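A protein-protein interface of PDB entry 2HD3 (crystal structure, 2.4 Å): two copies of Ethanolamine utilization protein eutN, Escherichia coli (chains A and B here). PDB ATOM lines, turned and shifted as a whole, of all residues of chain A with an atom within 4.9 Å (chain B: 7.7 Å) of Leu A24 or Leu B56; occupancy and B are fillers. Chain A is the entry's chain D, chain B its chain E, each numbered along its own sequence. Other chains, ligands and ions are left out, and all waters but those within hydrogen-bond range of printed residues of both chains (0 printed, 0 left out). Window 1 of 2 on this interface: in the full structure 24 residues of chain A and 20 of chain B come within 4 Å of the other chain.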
ATOM      1  N   GLY A   8     -23.179   9.620   2.262  1.00  0.00           N
ATOM      2  CA  GLY A   8     -22.048   9.977   1.415  1.00  0.00           C
ATOM      3  C   GLY A   8     -22.182  11.329   0.740  1.00  0.00           C
ATOM      4  O   GLY A   8     -22.953  12.178   1.195  1.00  0.00           O
ATOM      5  N   GLN A   9     -21.441  11.532  -0.350  1.00  0.00           N
ATOM      6  CA  GLN A   9     -21.477  12.807  -1.079  1.00  0.00           C
ATOM      7  C   GLN A   9     -21.162  12.722  -2.573  1.00  0.00           C
ATOM      8  O   GLN A   9     -20.371  11.894  -3.015  1.00  0.00           O
ATOM      9  CB  GLN A   9     -20.512  13.784  -0.422  1.00  0.00           C
ATOM     10  CG  GLN A   9     -19.122  13.228  -0.248  1.00  0.00           C
ATOM     11  CD  GLN A   9     -18.425  13.837   0.955  1.00  0.00           C
ATOM     12  OE1 GLN A   9     -18.896  13.704   2.092  1.00  0.00           O
ATOM     13  NE2 GLN A   9     -17.301  14.501   0.718  1.00  0.00           N
ATOM     14  N   ILE A  10     -21.788  13.589  -3.353  1.00  0.00           N
ATOM     15  CA  ILE A  10     -21.544  13.600  -4.787  1.00  0.00           C
ATOM     16  C   ILE A  10     -20.616  14.754  -5.125  1.00  0.00           C
ATOM     17  O   ILE A  10     -20.657  15.804  -4.486  1.00  0.00           O
ATOM     18  CB  ILE A  10     -22.862  13.772  -5.591  1.00  0.00           C
ATOM     19  CG1 ILE A  10     -23.696  12.506  -5.478  1.00  0.00           C
ATOM     20  CG2 ILE A  10     -22.580  14.097  -7.046  1.00  0.00           C
ATOM     21  CD1 ILE A  10     -24.681  12.540  -4.332  1.00  0.00           C
ATOM     22  N   CYS A  12     -19.575  17.147  -8.248  1.00  0.00           N
ATOM     23  CA  CYS A  12     -19.871  17.655  -9.578  1.00  0.00           C
ATOM     24  C   CYS A  12     -19.057  18.919  -9.833  1.00  0.00           C
ATOM     25  O   CYS A  12     -19.455  19.999  -9.401  1.00  0.00           O
ATOM     26  CB  CYS A  12     -21.342  18.034  -9.681  1.00  0.00           C
ATOM     27  SG  CYS A  12     -22.482  16.671  -9.752  1.00  0.00           S
ATOM     28  N   ARG A  15     -21.258  22.159 -12.631  1.00  0.00           N
ATOM     29  CA  ARG A  15     -22.601  22.171 -12.081  1.00  0.00           C
ATOM     30  C   ARG A  15     -23.253  23.550 -12.253  1.00  0.00           C
ATOM     31  O   ARG A  15     -22.577  24.520 -12.592  1.00  0.00           O
ATOM     32  CB  ARG A  15     -22.533  21.823 -10.592  1.00  0.00           C
ATOM     33  CG  ARG A  15     -22.020  22.957  -9.690  1.00  0.00           C
ATOM     34  CD  ARG A  15     -21.599  22.448  -8.290  1.00  0.00           C
ATOM     35  NE  ARG A  15     -22.111  23.268  -7.196  1.00  0.00           N
ATOM     36  CZ  ARG A  15     -22.213  22.860  -5.930  1.00  0.00           C
ATOM     37  NH1 ARG A  15     -22.706  23.677  -5.001  1.00  0.00           N
ATOM     38  NH2 ARG A  15     -21.827  21.634  -5.588  1.00  0.00           N
ATOM     39  N   ASP A  22     -22.062  24.950  -2.135  1.00  0.00           N
ATOM     40  CA  ASP A  22     -22.627  24.092  -1.120  1.00  0.00           C
ATOM     41  C   ASP A  22     -22.380  22.646  -1.502  1.00  0.00           C
ATOM     42  O   ASP A  22     -22.196  22.325  -2.676  1.00  0.00           O
ATOM     43  CB  ASP A  22     -24.117  24.365  -1.000  1.00  0.00           C
ATOM     44  CG  ASP A  22     -24.398  25.708  -0.375  1.00  0.00           C
ATOM     45  OD1 ASP A  22     -25.374  26.360  -0.795  1.00  0.00           O
ATOM     46  OD2 ASP A  22     -23.646  26.108   0.549  1.00  0.00           O
ATOM     47  N   LYS A  23     -22.377  21.778  -0.498  1.00  0.00           N
ATOM     48  CA  LYS A  23     -22.138  20.356  -0.696  1.00  0.00           C
ATOM     49  C   LYS A  23     -23.383  19.612  -1.201  1.00  0.00           C
ATOM     50  O   LYS A  23     -24.512  20.049  -0.975  1.00  0.00           O
ATOM     51  CB  LYS A  23     -21.670  19.748   0.630  1.00  0.00           C
ATOM     52  CG  LYS A  23     -20.361  18.975   0.554  1.00  0.00           C
ATOM     53  CD  LYS A  23     -19.151  19.879   0.335  1.00  0.00           C
ATOM     54  CE  LYS A  23     -18.827  20.722   1.570  1.00  0.00           C
ATOM     55  NZ  LYS A  23     -17.554  21.509   1.403  1.00  0.00           N
ATOM     56  N   LEU A  24     -23.159  18.494  -1.889  1.00  0.00           N
ATOM     57  CA  LEU A  24     -24.228  17.633  -2.425  1.00  0.00           C
ATOM     58  C   LEU A  24     -24.114  16.306  -1.701  1.00  0.00           C
ATOM     59  O   LEU A  24     -23.179  15.549  -1.930  1.00  0.00           O
ATOM     60  CB  LEU A  24     -24.024  17.405  -3.915  1.00  0.00           C
ATOM     61  CG  LEU A  24     -24.064  18.729  -4.654  1.00  0.00           C
ATOM     62  CD1 LEU A  24     -23.168  18.698  -5.885  1.00  0.00           C
ATOM     63  CD2 LEU A  24     -25.508  19.033  -4.995  1.00  0.00           C
ATOM     64  N   LEU A  25     -25.082  16.013  -0.851  1.00  0.00           N
ATOM     65  CA  LEU A  25     -25.031  14.799  -0.066  1.00  0.00           C
ATOM     66  C   LEU A  25     -25.970  13.668  -0.452  1.00  0.00           C
ATOM     67  O   LEU A  25     -27.112  13.886  -0.878  1.00  0.00           O
ATOM     68  CB  LEU A  25     -25.266  15.147   1.405  1.00  0.00           C
ATOM     69  CG  LEU A  25     -24.390  16.255   2.002  1.00  0.00           C
ATOM     70  CD1 LEU A  25     -24.850  16.553   3.418  1.00  0.00           C
ATOM     71  CD2 LEU A  25     -22.933  15.830   1.998  1.00  0.00           C
ATOM     72  N   MET A  26     -25.463  12.448  -0.295  1.00  0.00           N
ATOM     73  CA  MET A  26     -26.239  11.244  -0.546  1.00  0.00           C
ATOM     74  C   MET A  26     -27.053  11.074   0.730  1.00  0.00           C
ATOM     75  O   MET A  26     -26.477  11.081   1.811  1.00  0.00           O
ATOM     76  CB  MET A  26     -25.306  10.043  -0.696  1.00  0.00           C
ATOM     77  CG  MET A  26     -24.646   9.904  -2.046  1.00  0.00           C
ATOM     78  SD  MET A  26     -25.868   9.081  -3.294  1.00  0.00           S
ATOM     79  CE  MET A  26     -25.611   7.223  -2.787  1.00  0.00           C
ATOM     80  N   VAL A  42     -30.426  12.831  -3.364  1.00  0.00           N
ATOM     81  CA  VAL A  42     -29.320  13.770  -3.144  1.00  0.00           C
ATOM     82  C   VAL A  42     -29.869  15.120  -2.707  1.00  0.00           C
ATOM     83  O   VAL A  42     -30.742  15.688  -3.360  1.00  0.00           O
ATOM     84  CB  VAL A  42     -28.471  13.978  -4.430  1.00  0.00           C
ATOM     85  CG1 VAL A  42     -27.239  14.830  -4.116  1.00  0.00           C
ATOM     86  CG2 VAL A  42     -28.048  12.636  -4.995  1.00  0.00           C
ATOM     87  N   ALA A  43     -29.353  15.638  -1.604  1.00  0.00           N
ATOM     88  CA  ALA A  43     -29.814  16.916  -1.087  1.00  0.00           C
ATOM     89  C   ALA A  43     -28.669  17.903  -0.945  1.00  0.00           C
ATOM     90  O   ALA A  43     -27.538  17.512  -0.670  1.00  0.00           O
ATOM     91  CB  ALA A  43     -30.487  16.711   0.257  1.00  0.00           C
ATOM     92  N   ILE A  44     -28.974  19.183  -1.138  1.00  0.00           N
ATOM     93  CA  ILE A  44     -27.977  20.237  -1.016  1.00  0.00           C
ATOM     94  C   ILE A  44     -27.820  20.527   0.475  1.00  0.00           C
ATOM     95  O   ILE A  44     -28.783  20.444   1.244  1.00  0.00           O
ATOM     96  CB  ILE A  44     -28.416  21.531  -1.765  1.00  0.00           C
ATOM     97  CG1 ILE A  44     -27.247  22.502  -1.880  1.00  0.00           C
ATOM     98  CG2 ILE A  44     -29.540  22.232  -1.010  1.00  0.00           C
ATOM     99  CD1 ILE A  44     -26.098  21.978  -2.693  1.00  0.00           C
ATOM    100  N   MET B   1     -33.001  15.676  -5.115  1.00  0.00           N
ATOM    101  CA  MET B   1     -32.328  15.410  -6.424  1.00  0.00           C
ATOM    102  C   MET B   1     -31.990  13.938  -6.569  1.00  0.00           C
ATOM    103  O   MET B   1     -31.998  13.196  -5.598  1.00  0.00           O
ATOM    104  CB  MET B   1     -31.049  16.244  -6.543  1.00  0.00           C
ATOM    105  CG  MET B   1     -31.298  17.735  -6.692  1.00  0.00           C
ATOM    106  SD  MET B   1     -31.547  18.640  -4.999  1.00  0.00           S
ATOM    107  CE  MET B   1     -29.690  19.113  -4.708  1.00  0.00           C
ATOM    108  N   LYS B   2     -31.708  13.508  -7.788  1.00  0.00           N
ATOM    109  CA  LYS B   2     -31.354  12.110  -8.007  1.00  0.00           C
ATOM    110  C   LYS B   2     -30.382  11.909  -9.156  1.00  0.00           C
ATOM    111  O   LYS B   2     -30.356  12.680 -10.108  1.00  0.00           O
ATOM    112  CB  LYS B   2     -32.624  11.258  -8.210  1.00  0.00           C
ATOM    113  CG  LYS B   2     -33.690  11.890  -9.053  1.00  0.00           C
ATOM    114  CD  LYS B   2     -34.994  11.130  -8.911  1.00  0.00           C
ATOM    115  CE  LYS B   2     -36.061  11.668  -9.855  1.00  0.00           C
ATOM    116  NZ  LYS B   2     -37.347  10.910  -9.721  1.00  0.00           N
ATOM    117  N   LEU B   3     -29.563  10.876  -9.033  1.00  0.00           N
ATOM    118  CA  LEU B   3     -28.576  10.547 -10.039  1.00  0.00           C
ATOM    119  C   LEU B   3     -29.227   9.826 -11.215  1.00  0.00           C
ATOM    120  O   LEU B   3     -30.295   9.240 -11.076  1.00  0.00           O
ATOM    121  CB  LEU B   3     -27.506   9.648  -9.425  1.00  0.00           C
ATOM    122  CG  LEU B   3     -26.807  10.306  -8.255  1.00  0.00           C
ATOM    123  CD1 LEU B   3     -26.154   9.261  -7.363  1.00  0.00           C
ATOM    124  CD2 LEU B   3     -25.800  11.324  -8.791  1.00  0.00           C
ATOM    125  N   ALA B   4     -28.575   9.861 -12.373  1.00  0.00           N
ATOM    126  CA  ALA B   4     -29.099   9.181 -13.533  1.00  0.00           C
ATOM    127  C   ALA B   4     -28.005   9.138 -14.565  1.00  0.00           C
ATOM    128  O   ALA B   4     -27.000   9.831 -14.439  1.00  0.00           O
ATOM    129  CB  ALA B   4     -30.327   9.908 -14.078  1.00  0.00           C
ATOM    130  N   VAL B   5     -28.194   8.290 -15.568  1.00  0.00           N
ATOM    131  CA  VAL B   5     -27.242   8.132 -16.652  1.00  0.00           C
ATOM    132  C   VAL B   5     -27.920   8.636 -17.923  1.00  0.00           C
ATOM    133  O   VAL B   5     -29.147   8.581 -18.041  1.00  0.00           O
ATOM    134  CB  VAL B   5     -26.880   6.644 -16.878  1.00  0.00           C
ATOM    135  CG1 VAL B   5     -25.584   6.535 -17.659  1.00  0.00           C
ATOM    136  CG2 VAL B   5     -26.775   5.920 -15.559  1.00  0.00           C
ATOM    137  N   ALA B  43     -34.911  14.764 -19.970  1.00  0.00           N
ATOM    138  CA  ALA B  43     -34.567  15.952 -19.210  1.00  0.00           C
ATOM    139  C   ALA B  43     -33.980  17.033 -20.095  1.00  0.00           C
ATOM    140  O   ALA B  43     -33.401  16.738 -21.136  1.00  0.00           O
ATOM    141  CB  ALA B  43     -33.587  15.589 -18.117  1.00  0.00           C
ATOM    142  N   ILE B  44     -34.151  18.287 -19.686  1.00  0.00           N
ATOM    143  CA  ILE B  44     -33.597  19.388 -20.435  1.00  0.00           C
ATOM    144  C   ILE B  44     -32.170  19.597 -19.944  1.00  0.00           C
ATOM    145  O   ILE B  44     -31.902  19.551 -18.747  1.00  0.00           O
ATOM    146  CB  ILE B  44     -34.410  20.685 -20.264  1.00  0.00           C
ATOM    147  CG1 ILE B  44     -33.947  21.696 -21.315  1.00  0.00           C
ATOM    148  CG2 ILE B  44     -34.229  21.257 -18.870  1.00  0.00           C
ATOM    149  CD1 ILE B  44     -35.003  22.707 -21.707  1.00  0.00           C
ATOM    150  N   ILE B  47     -25.978  22.238 -19.937  1.00  0.00           N
ATOM    151  CA  ILE B  47     -24.667  22.184 -19.314  1.00  0.00           C
ATOM    152  C   ILE B  47     -23.688  21.477 -20.234  1.00  0.00           C
ATOM    153  O   ILE B  47     -22.474  21.592 -20.074  1.00  0.00           O
ATOM    154  CB  ILE B  47     -24.719  21.430 -17.980  1.00  0.00           C
ATOM    155  CG1 ILE B  47     -25.596  22.196 -16.996  1.00  0.00           C
ATOM    156  CG2 ILE B  47     -23.315  21.252 -17.412  1.00  0.00           C
ATOM    157  CD1 ILE B  47     -25.545  21.646 -15.600  1.00  0.00           C
ATOM    158  N   GLU B  53     -22.652   9.856 -19.518  1.00  0.00           N
ATOM    159  CA  GLU B  53     -22.294  10.641 -18.354  1.00  0.00           C
ATOM    160  C   GLU B  53     -23.370  10.568 -17.293  1.00  0.00           C
ATOM    161  O   GLU B  53     -24.566  10.423 -17.579  1.00  0.00           O
ATOM    162  CB  GLU B  53     -22.026  12.104 -18.729  1.00  0.00           C
ATOM    163  CG  GLU B  53     -20.827  12.299 -19.683  1.00  0.00           C
ATOM    164  CD  GLU B  53     -20.402  13.764 -19.822  1.00  0.00           C
ATOM    165  OE1 GLU B  53     -21.262  14.624 -20.086  1.00  0.00           O
ATOM    166  OE2 GLU B  53     -19.196  14.053 -19.675  1.00  0.00           O
ATOM    167  N   TRP B  54     -22.915  10.640 -16.049  1.00  0.00           N
ATOM    168  CA  TRP B  54     -23.786  10.607 -14.900  1.00  0.00           C
ATOM    169  C   TRP B  54     -24.099  12.057 -14.590  1.00  0.00           C
ATOM    170  O   TRP B  54     -23.213  12.917 -14.592  1.00  0.00           O
ATOM    171  CB  TRP B  54     -23.070   9.948 -13.735  1.00  0.00           C
ATOM    172  CG  TRP B  54     -23.192   8.466 -13.732  1.00  0.00           C
ATOM    173  CD1 TRP B  54     -23.165   7.636 -14.812  1.00  0.00           C
ATOM    174  CD2 TRP B  54     -23.320   7.628 -12.584  1.00  0.00           C
ATOM    175  NE1 TRP B  54     -23.272   6.325 -14.412  1.00  0.00           N
ATOM    176  CE2 TRP B  54     -23.370   6.289 -13.047  1.00  0.00           C
ATOM    177  CE3 TRP B  54     -23.408   7.876 -11.211  1.00  0.00           C
ATOM    178  CZ2 TRP B  54     -23.490   5.195 -12.175  1.00  0.00           C
ATOM    179  CZ3 TRP B  54     -23.530   6.794 -10.347  1.00  0.00           C
ATOM    180  CH2 TRP B  54     -23.572   5.468 -10.835  1.00  0.00           C
ATOM    181  N   VAL B  55     -25.373  12.316 -14.327  1.00  0.00           N
ATOM    182  CA  VAL B  55     -25.837  13.654 -14.051  1.00  0.00           C
ATOM    183  C   VAL B  55     -26.758  13.688 -12.858  1.00  0.00           C
ATOM    184  O   VAL B  55     -27.348  12.674 -12.481  1.00  0.00           O
ATOM    185  CB  VAL B  55     -26.598  14.208 -15.267  1.00  0.00           C
ATOM    186  CG1 VAL B  55     -25.710  14.133 -16.521  1.00  0.00           C
ATOM    187  CG2 VAL B  55     -27.859  13.390 -15.493  1.00  0.00           C
ATOM    188  N   LEU B  56     -26.864  14.870 -12.265  1.00  0.00           N
ATOM    189  CA  LEU B  56     -27.741  15.096 -11.137  1.00  0.00           C
ATOM    190  C   LEU B  56     -28.969  15.830 -11.676  1.00  0.00           C
ATOM    191  O   LEU B  56     -28.857  16.845 -12.367  1.00  0.00           O
ATOM    192  CB  LEU B  56     -27.051  15.938 -10.063  1.00  0.00           C
ATOM    193  CG  LEU B  56     -27.909  16.063  -8.794  1.00  0.00           C
ATOM    194  CD1 LEU B  56     -28.112  14.669  -8.203  1.00  0.00           C
ATOM    195  CD2 LEU B  56     -27.235  16.989  -7.779  1.00  0.00           C
ATOM    196  N   LEU B  57     -30.141  15.308 -11.336  1.00  0.00           N
ATOM    197  CA  LEU B  57     -31.384  15.871 -11.813  1.00  0.00           C
ATOM    198  C   LEU B  57     -32.235  16.514 -10.740  1.00  0.00           C
ATOM    199  O   LEU B  57     -32.305  16.019  -9.621  1.00  0.00           O
ATOM    200  CB  LEU B  57     -32.227  14.792 -12.516  1.00  0.00           C
ATOM    201  CG  LEU B  57     -31.625  14.048 -13.700  1.00  0.00           C
ATOM    202  CD1 LEU B  57     -32.660  13.098 -14.290  1.00  0.00           C
ATOM    203  CD2 LEU B  57     -31.164  15.039 -14.757  1.00  0.00           C
ATOM    204  N   VAL B  58     -32.888  17.614 -11.114  1.00  0.00           N
ATOM    205  CA  VAL B  58     -33.796  18.340 -10.248  1.00  0.00           C
ATOM    206  C   VAL B  58     -35.137  18.261 -11.001  1.00  0.00           C
ATOM    207  O   VAL B  58     -35.149  18.203 -12.242  1.00  0.00           O
ATOM    208  CB  VAL B  58     -33.373  19.818 -10.101  1.00  0.00           C
ATOM    209  CG1 VAL B  58     -33.538  20.551 -11.425  1.00  0.00           C
ATOM    210  CG2 VAL B  58     -34.198  20.492  -9.024  1.00  0.00           C
ATOM    211  N   LEU B  76     -37.946  18.391 -15.393  1.00  0.00           N
ATOM    212  CA  LEU B  76     -36.711  17.612 -15.226  1.00  0.00           C
ATOM    213  C   LEU B  76     -35.575  18.401 -15.865  1.00  0.00           C
ATOM    214  O   LEU B  76     -35.618  18.705 -17.059  1.00  0.00           O
ATOM    215  CB  LEU B  76     -36.784  16.271 -15.943  1.00  0.00           C
ATOM    216  CG  LEU B  76     -36.757  14.955 -15.166  1.00  0.00           C
ATOM    217  CD1 LEU B  76     -36.236  13.890 -16.120  1.00  0.00           C
ATOM    218  CD2 LEU B  76     -35.878  15.034 -13.928  1.00  0.00           C
ATOM    219  N   CYS B  77     -34.550  18.699 -15.072  1.00  0.00           N
ATOM    220  CA  CYS B  77     -33.421  19.469 -15.544  1.00  0.00           C
ATOM    221  C   CYS B  77     -32.090  19.020 -14.958  1.00  0.00           C
ATOM    222  O   CYS B  77     -31.983  18.769 -13.755  1.00  0.00           O
ATOM    223  CB  CYS B  77     -33.640  20.938 -15.192  1.00  0.00           C
ATOM    224  SG  CYS B  77     -32.401  22.051 -15.871  1.00  0.00           S
ATOM    225  N   VAL B  78     -31.076  18.927 -15.815  1.00  0.00           N
ATOM    226  CA  VAL B  78     -29.732  18.557 -15.379  1.00  0.00           C
ATOM    227  C   VAL B  78     -29.096  19.798 -14.739  1.00  0.00           C
ATOM    228  O   VAL B  78     -28.953  20.817 -15.414  1.00  0.00           O
ATOM    229  CB  VAL B  78     -28.822  18.178 -16.557  1.00  0.00           C
ATOM    230  CG1 VAL B  78     -27.488  17.696 -16.019  1.00  0.00           C
ATOM    231  CG2 VAL B  78     -29.468  17.126 -17.434  1.00  0.00           C
ATOM    232  N   ILE B  79     -28.732  19.722 -13.454  1.00  0.00           N
ATOM    233  CA  ILE B  79     -28.086  20.850 -12.762  1.00  0.00           C
ATOM    234  C   ILE B  79     -26.607  20.605 -12.457  1.00  0.00           C
ATOM    235  O   ILE B  79     -25.974  21.425 -11.793  1.00  0.00           O
ATOM    236  CB  ILE B  79     -28.764  21.198 -11.415  1.00  0.00           C
ATOM    237  CG1 ILE B  79     -28.688  19.997 -10.465  1.00  0.00           C
ATOM    238  CG2 ILE B  79     -30.193  21.669 -11.663  1.00  0.00           C
ATOM    239  CD1 ILE B  79     -29.284  20.254  -9.077  1.00  0.00           C
ATOM    240  N   GLY B  80     -26.072  19.478 -12.927  1.00  0.00           N
ATOM    241  CA  GLY B  80     -24.674  19.157 -12.705  1.00  0.00           C
ATOM    242  C   GLY B  80     -24.201  17.851 -13.342  1.00  0.00           C
ATOM    243  O   GLY B  80     -24.981  16.906 -13.506  1.00  0.00           O
ATOM    244  N   ILE B  81     -22.926  17.809 -13.723  1.00  0.00           N
ATOM    245  CA  ILE B  81     -22.313  16.611 -14.294  1.00  0.00           C
ATOM    246  C   ILE B  81     -21.555  15.949 -13.141  1.00  0.00           C
ATOM    247  O   ILE B  81     -20.738  16.585 -12.477  1.00  0.00           O
ATOM    248  CB  ILE B  81     -21.308  16.953 -15.433  1.00  0.00           C
ATOM    249  CG1 ILE B  81     -21.994  17.809 -16.507  1.00  0.00           C
ATOM    250  CG2 ILE B  81     -20.771  15.666 -16.072  1.00  0.00           C
ATOM    251  CD1 ILE B  81     -23.151  17.124 -17.213  1.00  0.00           C
ATOM    252  N   VAL B  82     -21.842  14.673 -12.913  1.00  0.00           N
ATOM    253  CA  VAL B  82     -21.254  13.894 -11.825  1.00  0.00           C
ATOM    254  C   VAL B  82     -19.838  13.380 -12.081  1.00  0.00           C
ATOM    255  O   VAL B  82     -19.576  12.746 -13.102  1.00  0.00           O
ATOM    256  CB  VAL B  82     -22.184  12.698 -11.506  1.00  0.00           C
ATOM    257  CG1 VAL B  82     -21.597  11.828 -10.397  1.00  0.00           C
ATOM    258  CG2 VAL B  82     -23.555  13.220 -11.109  1.00  0.00           C
ATOM    259  N   GLU B  84     -17.878  11.870  -9.258  1.00  0.00           N
ATOM    260  CA  GLU B  84     -17.740  10.704  -8.406  1.00  0.00           C
ATOM    261  C   GLU B  84     -18.843  10.654  -7.359  1.00  0.00           C
ATOM    262  O   GLU B  84     -19.353  11.690  -6.923  1.00  0.00           O
ATOM    263  CB  GLU B  84     -16.398  10.716  -7.697  1.00  0.00           C
ATOM    264  CG  GLU B  84     -16.264  11.831  -6.688  1.00  0.00           C
ATOM    265  CD  GLU B  84     -15.057  11.655  -5.787  1.00  0.00           C
ATOM    266  OE1 GLU B  84     -14.857  12.500  -4.891  1.00  0.00           O
ATOM    267  OE2 GLU B  84     -14.309  10.672  -5.971  1.00  0.00           O
ATOM    268  N   VAL B  86     -19.655   8.836  -3.652  1.00  0.00           N
ATOM    269  CA  VAL B  86     -19.179   8.078  -2.514  1.00  0.00           C
ATOM    270  C   VAL B  86     -20.352   7.836  -1.575  1.00  0.00           C
ATOM    271  O   VAL B  86     -21.023   8.773  -1.134  1.00  0.00           O
ATOM    272  CB  VAL B  86     -18.050   8.826  -1.783  1.00  0.00           C
ATOM    273  CG1 VAL B  86     -17.727   8.137  -0.474  1.00  0.00           C
ATOM    274  CG2 VAL B  86     -16.821   8.857  -2.666  1.00  0.00           C
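Hydrophobic or aromatic side chains of chain B within 4 Å of the printed part of chain A: Met B1, Leu B56 and Val B82. Of the 13 printed residues of chain A, 9 touch a printed residue of chain B. Hydrophobic or aromatic side chains of chain A within 4 Å of the printed part of chain B: Leu A24, Met A26 and Val A42. Among the printed residues, 12 pairs touch across the chains.
Of chain B, only Leu B56 comes within 4 Å of Leu A24. Leu B56 touches just these residues of chain A: Leu A24 and Val A42. Of the printed residues of chain A, Gly B80 touches Arg A15 (3.7 Å). Printed residues of chain B within 4 Å of Ile A10: Glu B84 (3.6 Å). Of the printed residues of chain A, Ile B79 touches Arg A15. Printed residues of chain B within 4 Å of Gln A9: Val B86. Printed residues of chain B within 4 Å of Cys A12: Ile B81 and Val B82. Ala A43 touches none of the printed residues of chain B. The nearest residue of chain B that does not touch Leu A24 is Met B1 (4.2 Å). The nearest printed residue of chain B that does not touch Ile A44 is Leu B56 (7.2 Å).
The backbone NH of Val B82 is in hydrogen-bond range of the backbone carbonyl oxygen of Trp B54, at 2.8 Å. The backbone carbonyl oxygen (O) of Gly A8 lies within hydrogen-bond range of the backbone NH (N) of Met A26 (2.9 Å). The backbone carbonyl oxygen of Gly B80 sits at hydrogen-bond distance from the backbone NH of Leu B56 (3.0 Å). The guanidinium group (NH1) of Arg A15 sits at hydrogen-bond distance from the backbone carbonyl oxygen (O) of Asp A22, at 2.7 Å. The backbone NH of Ile A10 lies within hydrogen-bond range of the backbone carbonyl oxygen of Leu A24 (2.8 Å). The backbone carbonyl oxygen (O) of Leu B56 sits at hydrogen-bond distance from the backbone NH (N) of Ile B79 (3.1 Å).
N of Val A42 lies within hydrogen-bond range of O of Met B1, 2.8 Å away. The backbone NH of Gln A9 is in hydrogen-bond range of the backbone carbonyl oxygen of Val B86 (2.9 Å). SG of Cys A12 lies close to N of Val B82 (3.8 Å). SG of Cys A12 sits close to O of Ile B81.
Gly A8 touches Val B86 (CA to O, 3.0 Å). CA of Ile A10 touches O of Glu B84, 3.6 Å away. Arg A15 touches Ile B79. Gly B80 touches Arg A15 (CA to CA, 3.7 Å). CD2 of Leu A24 touches CD2 of Leu B56, at 3.9 Å. O of Val B86 touches CG of Met A26, at 3.9 Å. Leu B56 touches Val A42 (CD1 to CG2, 3.8 Å). Ile A44 touches Met B1.
Positions printed for both chains: 43 and 44. Of the 12 pairs that touch across the chains among the printed residues, none has its exchanged pair printed and touching as well.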
